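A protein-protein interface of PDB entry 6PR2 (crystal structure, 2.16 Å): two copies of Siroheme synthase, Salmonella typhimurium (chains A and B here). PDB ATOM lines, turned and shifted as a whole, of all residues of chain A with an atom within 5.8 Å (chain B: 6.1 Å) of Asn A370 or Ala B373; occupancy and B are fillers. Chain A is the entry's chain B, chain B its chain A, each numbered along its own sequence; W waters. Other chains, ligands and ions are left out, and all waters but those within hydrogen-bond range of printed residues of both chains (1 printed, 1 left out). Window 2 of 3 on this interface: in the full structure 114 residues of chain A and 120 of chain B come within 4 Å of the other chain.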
ATOM      1  N   ARG A 354      -7.815 -12.659  -5.804  1.00  0.00           N
ATOM      2  CA  ARG A 354      -6.415 -12.279  -5.916  1.00  0.00           C
ATOM      3  C   ARG A 354      -5.663 -13.369  -6.664  1.00  0.00           C
ATOM      4  O   ARG A 354      -5.598 -14.513  -6.197  1.00  0.00           O
ATOM      5  CB  ARG A 354      -5.791 -12.046  -4.541  1.00  0.00           C
ATOM      6  CG  ARG A 354      -4.641 -11.091  -4.600  1.00  0.00           C
ATOM      7  CD  ARG A 354      -3.894 -11.060  -3.299  1.00  0.00           C
ATOM      8  NE  ARG A 354      -2.629 -10.354  -3.449  1.00  0.00           N
ATOM      9  CZ  ARG A 354      -2.338  -9.208  -2.853  1.00  0.00           C
ATOM     10  NH1 ARG A 354      -3.218  -8.645  -2.049  1.00  0.00           N
ATOM     11  NH2 ARG A 354      -1.158  -8.638  -3.052  1.00  0.00           N
ATOM     12  N   ASP A 367       3.195  -9.369   0.484  1.00  0.00           N
ATOM     13  CA  ASP A 367       2.631  -8.650   1.626  1.00  0.00           C
ATOM     14  C   ASP A 367       1.698  -9.605   2.365  1.00  0.00           C
ATOM     15  O   ASP A 367       0.538  -9.783   1.981  1.00  0.00           O
ATOM     16  CB  ASP A 367       1.900  -7.395   1.155  1.00  0.00           C
ATOM     17  CG  ASP A 367       1.842  -6.306   2.223  1.00  0.00           C
ATOM     18  OD1 ASP A 367       1.851  -6.642   3.428  1.00  0.00           O
ATOM     19  OD2 ASP A 367       1.783  -5.112   1.850  1.00  0.00           O
ATOM     20  N   TRP A 368       2.199 -10.220   3.441  1.00  0.00           N
ATOM     21  CA  TRP A 368       1.473 -11.325   4.063  1.00  0.00           C
ATOM     22  C   TRP A 368       0.235 -10.849   4.816  1.00  0.00           C
ATOM     23  O   TRP A 368      -0.821 -11.494   4.751  1.00  0.00           O
ATOM     24  CB  TRP A 368       2.403 -12.109   4.984  1.00  0.00           C
ATOM     25  CG  TRP A 368       3.341 -12.962   4.218  1.00  0.00           C
ATOM     26  CD1 TRP A 368       4.695 -12.823   4.125  1.00  0.00           C
ATOM     27  CD2 TRP A 368       2.990 -14.073   3.389  1.00  0.00           C
ATOM     28  NE1 TRP A 368       5.208 -13.792   3.302  1.00  0.00           N
ATOM     29  CE2 TRP A 368       4.182 -14.573   2.840  1.00  0.00           C
ATOM     30  CE3 TRP A 368       1.780 -14.699   3.066  1.00  0.00           C
ATOM     31  CZ2 TRP A 368       4.202 -15.672   1.986  1.00  0.00           C
ATOM     32  CZ3 TRP A 368       1.800 -15.785   2.220  1.00  0.00           C
ATOM     33  CH2 TRP A 368       3.002 -16.262   1.687  1.00  0.00           C
ATOM     34  N   GLU A 369       0.345  -9.734   5.545  1.00  0.00           N
ATOM     35  CA  GLU A 369      -0.832  -9.172   6.203  1.00  0.00           C
ATOM     36  C   GLU A 369      -1.944  -8.911   5.197  1.00  0.00           C
ATOM     37  O   GLU A 369      -3.117  -9.191   5.470  1.00  0.00           O
ATOM     38  CB  GLU A 369      -0.464  -7.883   6.941  1.00  0.00           C
ATOM     39  CG  GLU A 369      -1.647  -7.133   7.548  1.00  0.00           C
ATOM     40  CD  GLU A 369      -2.030  -7.641   8.936  1.00  0.00           C
ATOM     41  OE1 GLU A 369      -1.492  -8.687   9.369  1.00  0.00           O
ATOM     42  OE2 GLU A 369      -2.861  -6.983   9.601  1.00  0.00           O
ATOM     43  N   ASN A 370      -1.587  -8.379   4.023  1.00  0.00           N
ATOM     44  CA  ASN A 370      -2.582  -8.120   2.987  1.00  0.00           C
ATOM     45  C   ASN A 370      -3.194  -9.423   2.475  1.00  0.00           C
ATOM     46  O   ASN A 370      -4.413  -9.512   2.299  1.00  0.00           O
ATOM     47  CB  ASN A 370      -1.962  -7.316   1.839  1.00  0.00           C
ATOM     48  CG  ASN A 370      -1.980  -5.801   2.098  1.00  0.00           C
ATOM     49  OD1 ASN A 370      -2.850  -5.281   2.806  1.00  0.00           O
ATOM     50  ND2 ASN A 370      -1.018  -5.091   1.511  1.00  0.00           N
ATOM     51  N   LEU A 371      -2.376 -10.456   2.258  1.00  0.00           N
ATOM     52  CA  LEU A 371      -2.939 -11.717   1.781  1.00  0.00           C
ATOM     53  C   LEU A 371      -3.841 -12.367   2.827  1.00  0.00           C
ATOM     54  O   LEU A 371      -4.806 -13.052   2.465  1.00  0.00           O
ATOM     55  CB  LEU A 371      -1.822 -12.668   1.357  1.00  0.00           C
ATOM     56  CG  LEU A 371      -1.177 -12.312   0.015  1.00  0.00           C
ATOM     57  CD1 LEU A 371       0.309 -12.601   0.046  1.00  0.00           C
ATOM     58  CD2 LEU A 371      -1.835 -13.064  -1.122  1.00  0.00           C
ATOM     59  N   ALA A 372      -3.579 -12.128   4.121  1.00  0.00           N
ATOM     60  CA  ALA A 372      -4.320 -12.802   5.179  1.00  0.00           C
ATOM     61  C   ALA A 372      -5.715 -12.233   5.406  1.00  0.00           C
ATOM     62  O   ALA A 372      -6.502 -12.853   6.131  1.00  0.00           O
ATOM     63  CB  ALA A 372      -3.534 -12.747   6.491  1.00  0.00           C
ATOM     64  N   ALA A 373      -6.044 -11.092   4.809  1.00  0.00           N
ATOM     65  CA  ALA A 373      -7.282 -10.407   5.150  1.00  0.00           C
ATOM     66  C   ALA A 373      -8.490 -11.200   4.656  1.00  0.00           C
ATOM     67  O   ALA A 373      -8.391 -12.054   3.772  1.00  0.00           O
ATOM     68  CB  ALA A 373      -7.293  -8.998   4.562  1.00  0.00           C
ATOM     69  N   GLN A 376     -11.584 -12.669   0.739  1.00  0.00           N
ATOM     70  CA  GLN A 376     -10.833 -12.835  -0.498  1.00  0.00           C
ATOM     71  C   GLN A 376     -10.864 -14.288  -0.943  1.00  0.00           C
ATOM     72  O   GLN A 376     -10.907 -15.205  -0.122  1.00  0.00           O
ATOM     73  CB  GLN A 376      -9.369 -12.457  -0.331  1.00  0.00           C
ATOM     74  CG  GLN A 376      -9.087 -11.059   0.156  1.00  0.00           C
ATOM     75  CD  GLN A 376      -7.597 -10.830   0.176  1.00  0.00           C
ATOM     76  OE1 GLN A 376      -6.998 -10.536  -0.859  1.00  0.00           O
ATOM     77  NE2 GLN A 376      -6.978 -11.027   1.332  1.00  0.00           N
ATOM     78  N   GLN B 351       2.813  -7.554  -8.916  1.00  0.00           N
ATOM     79  CA  GLN B 351       2.930  -8.850  -8.253  1.00  0.00           C
ATOM     80  C   GLN B 351       1.655  -9.669  -8.427  1.00  0.00           C
ATOM     81  O   GLN B 351       1.709 -10.901  -8.543  1.00  0.00           O
ATOM     82  CB  GLN B 351       3.238  -8.644  -6.756  1.00  0.00           C
ATOM     83  CG  GLN B 351       1.982  -8.646  -5.869  1.00  0.00           C
ATOM     84  CD  GLN B 351       2.126  -7.998  -4.504  1.00  0.00           C
ATOM     85  OE1 GLN B 351       2.902  -8.449  -3.659  1.00  0.00           O
ATOM     86  NE2 GLN B 351       1.348  -6.942  -4.273  1.00  0.00           N
ATOM     87  N   ARG B 354      -5.901  -8.068  -8.753  1.00  0.00           N
ATOM     88  CA  ARG B 354      -7.114  -8.125  -7.958  1.00  0.00           C
ATOM     89  C   ARG B 354      -8.311  -7.848  -8.853  1.00  0.00           C
ATOM     90  O   ARG B 354      -8.397  -6.785  -9.476  1.00  0.00           O
ATOM     91  CB  ARG B 354      -7.068  -7.117  -6.811  1.00  0.00           C
ATOM     92  CG  ARG B 354      -5.874  -7.258  -5.957  1.00  0.00           C
ATOM     93  CD  ARG B 354      -6.029  -6.360  -4.767  1.00  0.00           C
ATOM     94  NE  ARG B 354      -7.005  -6.900  -3.838  1.00  0.00           N
ATOM     95  CZ  ARG B 354      -6.734  -7.129  -2.568  1.00  0.00           C
ATOM     96  NH1 ARG B 354      -5.522  -6.856  -2.114  1.00  0.00           N
ATOM     97  NH2 ARG B 354      -7.662  -7.627  -1.766  1.00  0.00           N
ATOM     98  N   ASP B 367     -12.019  -3.251   1.646  1.00  0.00           N
ATOM     99  CA  ASP B 367     -10.832  -3.138   2.501  1.00  0.00           C
ATOM    100  C   ASP B 367      -9.792  -2.296   1.768  1.00  0.00           C
ATOM    101  O   ASP B 367      -8.928  -2.817   1.057  1.00  0.00           O
ATOM    102  CB  ASP B 367     -10.282  -4.516   2.846  1.00  0.00           C
ATOM    103  CG  ASP B 367      -9.159  -4.461   3.872  1.00  0.00           C
ATOM    104  OD1 ASP B 367      -8.980  -3.405   4.518  1.00  0.00           O
ATOM    105  OD2 ASP B 367      -8.443  -5.474   4.019  1.00  0.00           O
ATOM    106  N   TRP B 368      -9.870  -0.973   1.969  1.00  0.00           N
ATOM    107  CA  TRP B 368      -9.178  -0.024   1.100  1.00  0.00           C
ATOM    108  C   TRP B 368      -7.675  -0.007   1.350  1.00  0.00           C
ATOM    109  O   TRP B 368      -6.896   0.187   0.407  1.00  0.00           O
ATOM    110  CB  TRP B 368      -9.770   1.376   1.284  1.00  0.00           C
ATOM    111  CG  TRP B 368     -11.177   1.475   0.794  1.00  0.00           C
ATOM    112  CD1 TRP B 368     -12.309   1.624   1.551  1.00  0.00           C
ATOM    113  CD2 TRP B 368     -11.611   1.421  -0.570  1.00  0.00           C
ATOM    114  NE1 TRP B 368     -13.418   1.680   0.737  1.00  0.00           N
ATOM    115  CE2 TRP B 368     -13.017   1.555  -0.568  1.00  0.00           C
ATOM    116  CE3 TRP B 368     -10.944   1.291  -1.796  1.00  0.00           C
ATOM    117  CZ2 TRP B 368     -13.767   1.554  -1.742  1.00  0.00           C
ATOM    118  CZ3 TRP B 368     -11.691   1.279  -2.961  1.00  0.00           C
ATOM    119  CH2 TRP B 368     -13.088   1.409  -2.925  1.00  0.00           C
ATOM    120  N   GLU B 369      -7.249  -0.199   2.604  1.00  0.00           N
ATOM    121  CA  GLU B 369      -5.830  -0.426   2.889  1.00  0.00           C
ATOM    122  C   GLU B 369      -5.294  -1.567   2.049  1.00  0.00           C
ATOM    123  O   GLU B 369      -4.195  -1.487   1.481  1.00  0.00           O
ATOM    124  CB  GLU B 369      -5.604  -0.771   4.366  1.00  0.00           C
ATOM    125  CG  GLU B 369      -6.364   0.056   5.369  1.00  0.00           C
ATOM    126  CD  GLU B 369      -7.841  -0.295   5.449  1.00  0.00           C
ATOM    127  OE1 GLU B 369      -8.228  -1.018   6.393  1.00  0.00           O
ATOM    128  OE2 GLU B 369      -8.613   0.131   4.565  1.00  0.00           O
ATOM    129  N   ASN B 370      -6.055  -2.656   1.981  1.00  0.00           N
ATOM    130  CA  ASN B 370      -5.617  -3.811   1.213  1.00  0.00           C
ATOM    131  C   ASN B 370      -5.502  -3.460  -0.263  1.00  0.00           C
ATOM    132  O   ASN B 370      -4.513  -3.802  -0.928  1.00  0.00           O
ATOM    133  CB  ASN B 370      -6.602  -4.956   1.426  1.00  0.00           C
ATOM    134  CG  ASN B 370      -5.926  -6.288   1.531  1.00  0.00           C
ATOM    135  OD1 ASN B 370      -5.369  -6.794   0.558  1.00  0.00           O
ATOM    136  ND2 ASN B 370      -5.962  -6.870   2.716  1.00  0.00           N
ATOM    137  N   LEU B 371      -6.507  -2.757  -0.788  1.00  0.00           N
ATOM    138  CA  LEU B 371      -6.561  -2.501  -2.224  1.00  0.00           C
ATOM    139  C   LEU B 371      -5.529  -1.470  -2.646  1.00  0.00           C
ATOM    140  O   LEU B 371      -5.136  -1.438  -3.817  1.00  0.00           O
ATOM    141  CB  LEU B 371      -7.948  -2.005  -2.628  1.00  0.00           C
ATOM    142  CG  LEU B 371      -9.146  -2.946  -2.452  1.00  0.00           C
ATOM    143  CD1 LEU B 371     -10.453  -2.223  -2.785  1.00  0.00           C
ATOM    144  CD2 LEU B 371      -8.979  -4.133  -3.341  1.00  0.00           C
ATOM    145  N   ALA B 372      -5.117  -0.596  -1.726  1.00  0.00           N
ATOM    146  CA  ALA B 372      -4.205   0.480  -2.068  1.00  0.00           C
ATOM    147  C   ALA B 372      -2.748   0.034  -2.144  1.00  0.00           C
ATOM    148  O   ALA B 372      -1.911   0.817  -2.608  1.00  0.00           O
ATOM    149  CB  ALA B 372      -4.343   1.616  -1.055  1.00  0.00           C
ATOM    150  N   ALA B 373      -2.437  -1.194  -1.718  1.00  0.00           N
ATOM    151  CA  ALA B 373      -1.062  -1.678  -1.674  1.00  0.00           C
ATOM    152  C   ALA B 373      -0.398  -1.619  -3.050  1.00  0.00           C
ATOM    153  O   ALA B 373      -1.040  -1.810  -4.091  1.00  0.00           O
ATOM    154  CB  ALA B 373      -1.029  -3.115  -1.145  1.00  0.00           C
ATOM    155  N   GLU B 374       0.917  -1.377  -3.038  1.00  0.00           N
ATOM    156  CA  GLU B 374       1.703  -1.209  -4.252  1.00  0.00           C
ATOM    157  C   GLU B 374       1.919  -2.545  -4.974  1.00  0.00           C
ATOM    158  O   GLU B 374       1.713  -3.633  -4.424  1.00  0.00           O
ATOM    159  CB  GLU B 374       3.055  -0.560  -3.936  1.00  0.00           C
ATOM    160  CG  GLU B 374       2.943   0.904  -3.494  1.00  0.00           C
ATOM    161  CD  GLU B 374       4.296   1.600  -3.311  1.00  0.00           C
ATOM    162  OE1 GLU B 374       4.301   2.796  -2.949  1.00  0.00           O
ATOM    163  OE2 GLU B 374       5.350   0.967  -3.535  1.00  0.00           O
ATOM    164  N   LYS B 375       2.348  -2.433  -6.235  1.00  0.00           N
ATOM    165  CA  LYS B 375       2.739  -3.569  -7.060  1.00  0.00           C
ATOM    166  C   LYS B 375       1.560  -4.504  -7.341  1.00  0.00           C
ATOM    167  O   LYS B 375       1.711  -5.728  -7.400  1.00  0.00           O
ATOM    168  CB  LYS B 375       3.910  -4.330  -6.432  1.00  0.00           C
ATOM    169  CG  LYS B 375       5.215  -3.509  -6.284  1.00  0.00           C
ATOM    170  CD  LYS B 375       5.975  -3.369  -7.604  1.00  0.00           C
ATOM    171  CE  LYS B 375       7.413  -2.882  -7.379  1.00  0.00           C
ATOM    172  NZ  LYS B 375       8.271  -3.144  -8.572  1.00  0.00           N
ATOM    173  N   GLN B 376       0.370  -3.940  -7.536  1.00  0.00           N
ATOM    174  CA  GLN B 376      -0.726  -4.761  -8.033  1.00  0.00           C
ATOM    175  C   GLN B 376      -1.500  -4.022  -9.108  1.00  0.00           C
ATOM    176  O   GLN B 376      -1.416  -2.805  -9.257  1.00  0.00           O
ATOM    177  CB  GLN B 376      -1.681  -5.234  -6.930  1.00  0.00           C
ATOM    178  CG  GLN B 376      -2.017  -4.280  -5.846  1.00  0.00           C
ATOM    179  CD  GLN B 376      -2.830  -4.953  -4.736  1.00  0.00           C
ATOM    180  OE1 GLN B 376      -3.006  -6.173  -4.734  1.00  0.00           O
ATOM    181  NE2 GLN B 376      -3.343  -4.155  -3.806  1.00  0.00           N
ATOM    182  N   LEU B 378      -5.336  -3.458 -10.094  1.00  0.00           N
ATOM    183  CA  LEU B 378      -6.714  -3.553  -9.616  1.00  0.00           C
ATOM    184  C   LEU B 378      -7.652  -3.523 -10.804  1.00  0.00           C
ATOM    185  O   LEU B 378      -7.515  -2.663 -11.681  1.00  0.00           O
ATOM    186  CB  LEU B 378      -7.084  -2.398  -8.680  1.00  0.00           C
ATOM    187  CG  LEU B 378      -6.152  -2.057  -7.536  1.00  0.00           C
ATOM    188  CD1 LEU B 378      -6.787  -0.883  -6.724  1.00  0.00           C
ATOM    189  CD2 LEU B 378      -5.939  -3.291  -6.658  1.00  0.00           C
ATOM    190  N   PHE B 397      -5.939   6.020   1.253  1.00  0.00           N
ATOM    191  CA  PHE B 397      -5.167   4.935   1.832  1.00  0.00           C
ATOM    192  C   PHE B 397      -3.789   4.806   1.193  1.00  0.00           C
ATOM    193  O   PHE B 397      -3.130   3.781   1.360  1.00  0.00           O
ATOM    194  CB  PHE B 397      -5.989   3.640   1.797  1.00  0.00           C
ATOM    195  CG  PHE B 397      -6.976   3.574   2.929  1.00  0.00           C
ATOM    196  CD1 PHE B 397      -8.257   4.074   2.776  1.00  0.00           C
ATOM    197  CD2 PHE B 397      -6.590   3.110   4.182  1.00  0.00           C
ATOM    198  CE1 PHE B 397      -9.167   4.069   3.848  1.00  0.00           C
ATOM    199  CE2 PHE B 397      -7.489   3.083   5.254  1.00  0.00           C
ATOM    200  CZ  PHE B 397      -8.778   3.573   5.094  1.00  0.00           C
ATOM    201  N   MET B 399      -2.429   5.361  -2.104  1.00  0.00           N
ATOM    202  CA  MET B 399      -2.023   5.168  -3.487  1.00  0.00           C
ATOM    203  C   MET B 399      -1.527   6.486  -4.067  1.00  0.00           C
ATOM    204  O   MET B 399      -2.090   7.546  -3.803  1.00  0.00           O
ATOM    205  CB  MET B 399      -3.172   4.611  -4.322  1.00  0.00           C
ATOM    206  CG  MET B 399      -2.760   4.317  -5.750  1.00  0.00           C
ATOM    207  SD  MET B 399      -3.998   3.388  -6.685  1.00  0.00           S
ATOM    208  CE  MET B 399      -3.776   1.783  -5.875  1.00  0.00           C
HETATM  209  O   HOH W   1      -0.147  -7.079  -1.354  1.00  0.00           O
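Arg A354 touches Asn B370, but with the chains exchanged Asn A370 does not touch Arg B354 (5.3 Å). Arg A354 touches Gln B376, and with the chains exchanged Gln A376 touches Arg B354. Asn B370 touches its own counterpart, Asn A370. Ala A373 touches Asp B367, but with the chains exchanged Asp A367 does not touch Ala B373 (4.6 Å). Of the 9 pairs that touch across the chains among the printed residues, 6 have their exchanged pair printed and touching as well.
Water W1 lies within hydrogen-bond range of the guanidinium group (NH2) of Arg A354 (2.5 Å) and the side-chain amide nitrogen (NE2) of Gln B351 (3.3 Å).
The side-chain amide nitrogen (NE2) of Gln B351 sits close to the guanidinium group (NH2) of Arg A354 (3.3 Å). The side-chain amide nitrogen (ND2) of Asn B370 is in hydrogen-bond range of the backbone carbonyl oxygen (O) of Asn A370. The guanidinium group of Arg A354 sits close to the guanidinium group of Arg B354 (2.9 Å). The guanidinium group (NH2) of Arg B354 lies within hydrogen-bond range of the side-chain amide oxygen (OE1) of Gln A376, at 3.1 Å.
Of the 15 printed residues of chain B, 6 touch a printed residue of chain A. Printed residues of chain B that touch a printed residue of chain A: Gln B351, Arg B354, Asp B367, Asn B370, Ala B373 and Gln B376. Hydrophobic or aromatic side chains of chain B within 4 Å of the printed part of chain A: Ala B373. Of the 9 printed residues of chain A, 4 touch a printed residue of chain B. Hydrophobic or aromatic side chains of chain A within 4 Å of the printed part of chain B: Ala A373. Among the printed residues, 9 pairs touch across the chains. Among the printed residues, no Asp or Glu carboxylate lies within 4 Å of a Lys or Arg side-chain nitrogen of the other chain.
Of the printed residues of chain B, Asn A370 touches Asn B370 (3.1 Å) and Ala B373 (3.3 Å). Of the printed residues of chain B, Ala A373 touches Asp B367 (3.7 Å) and Asn B370 (3.1 Å). Of the printed residues of chain A, Arg B354 touches Arg A354 and Gln A376. Of chain A, only Asn A370 comes within 4 Å of Ala B373. The nearest residue of chain B that does not touch Asn A370 is Glu B369 (4.2 Å).
The backbone carbonyl oxygen (O) of Leu A371 lies within hydrogen-bond range of the side-chain amide nitrogen (NE2) of Gln A376. The side-chain amide nitrogen (NE2) of Gln B376 is in hydrogen-bond range of the backbone carbonyl oxygen (O) of Leu B371 (3.3 Å). The side-chain carboxylate (OD2) of Asp A367 lies within hydrogen-bond range of the side-chain amide nitrogen (ND2) of Asn A370. The side-chain amide nitrogen (NE2) of Gln B376 sits close to the backbone carbonyl oxygen (O) of Ala B373 (3.3 Å). O of Asn A370 lies within hydrogen-bond range of NE2 of Gln A376 (3.1 Å). The side-chain amide nitrogen of Asn B370 is in hydrogen-bond range of the side-chain carboxylate of Asp B367 (3.1 Å).
NH1 of Arg A354 touches OD1 of Asn B370, at 3.9 Å. Gln B376 touches Arg A354. ND2 of Asn A370 touches CB of Ala B373, at 3.3 Å. OD2 of Asp B367 touches CB of Ala A373, at 3.7 Å. Ala A373 touches Asn B370.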
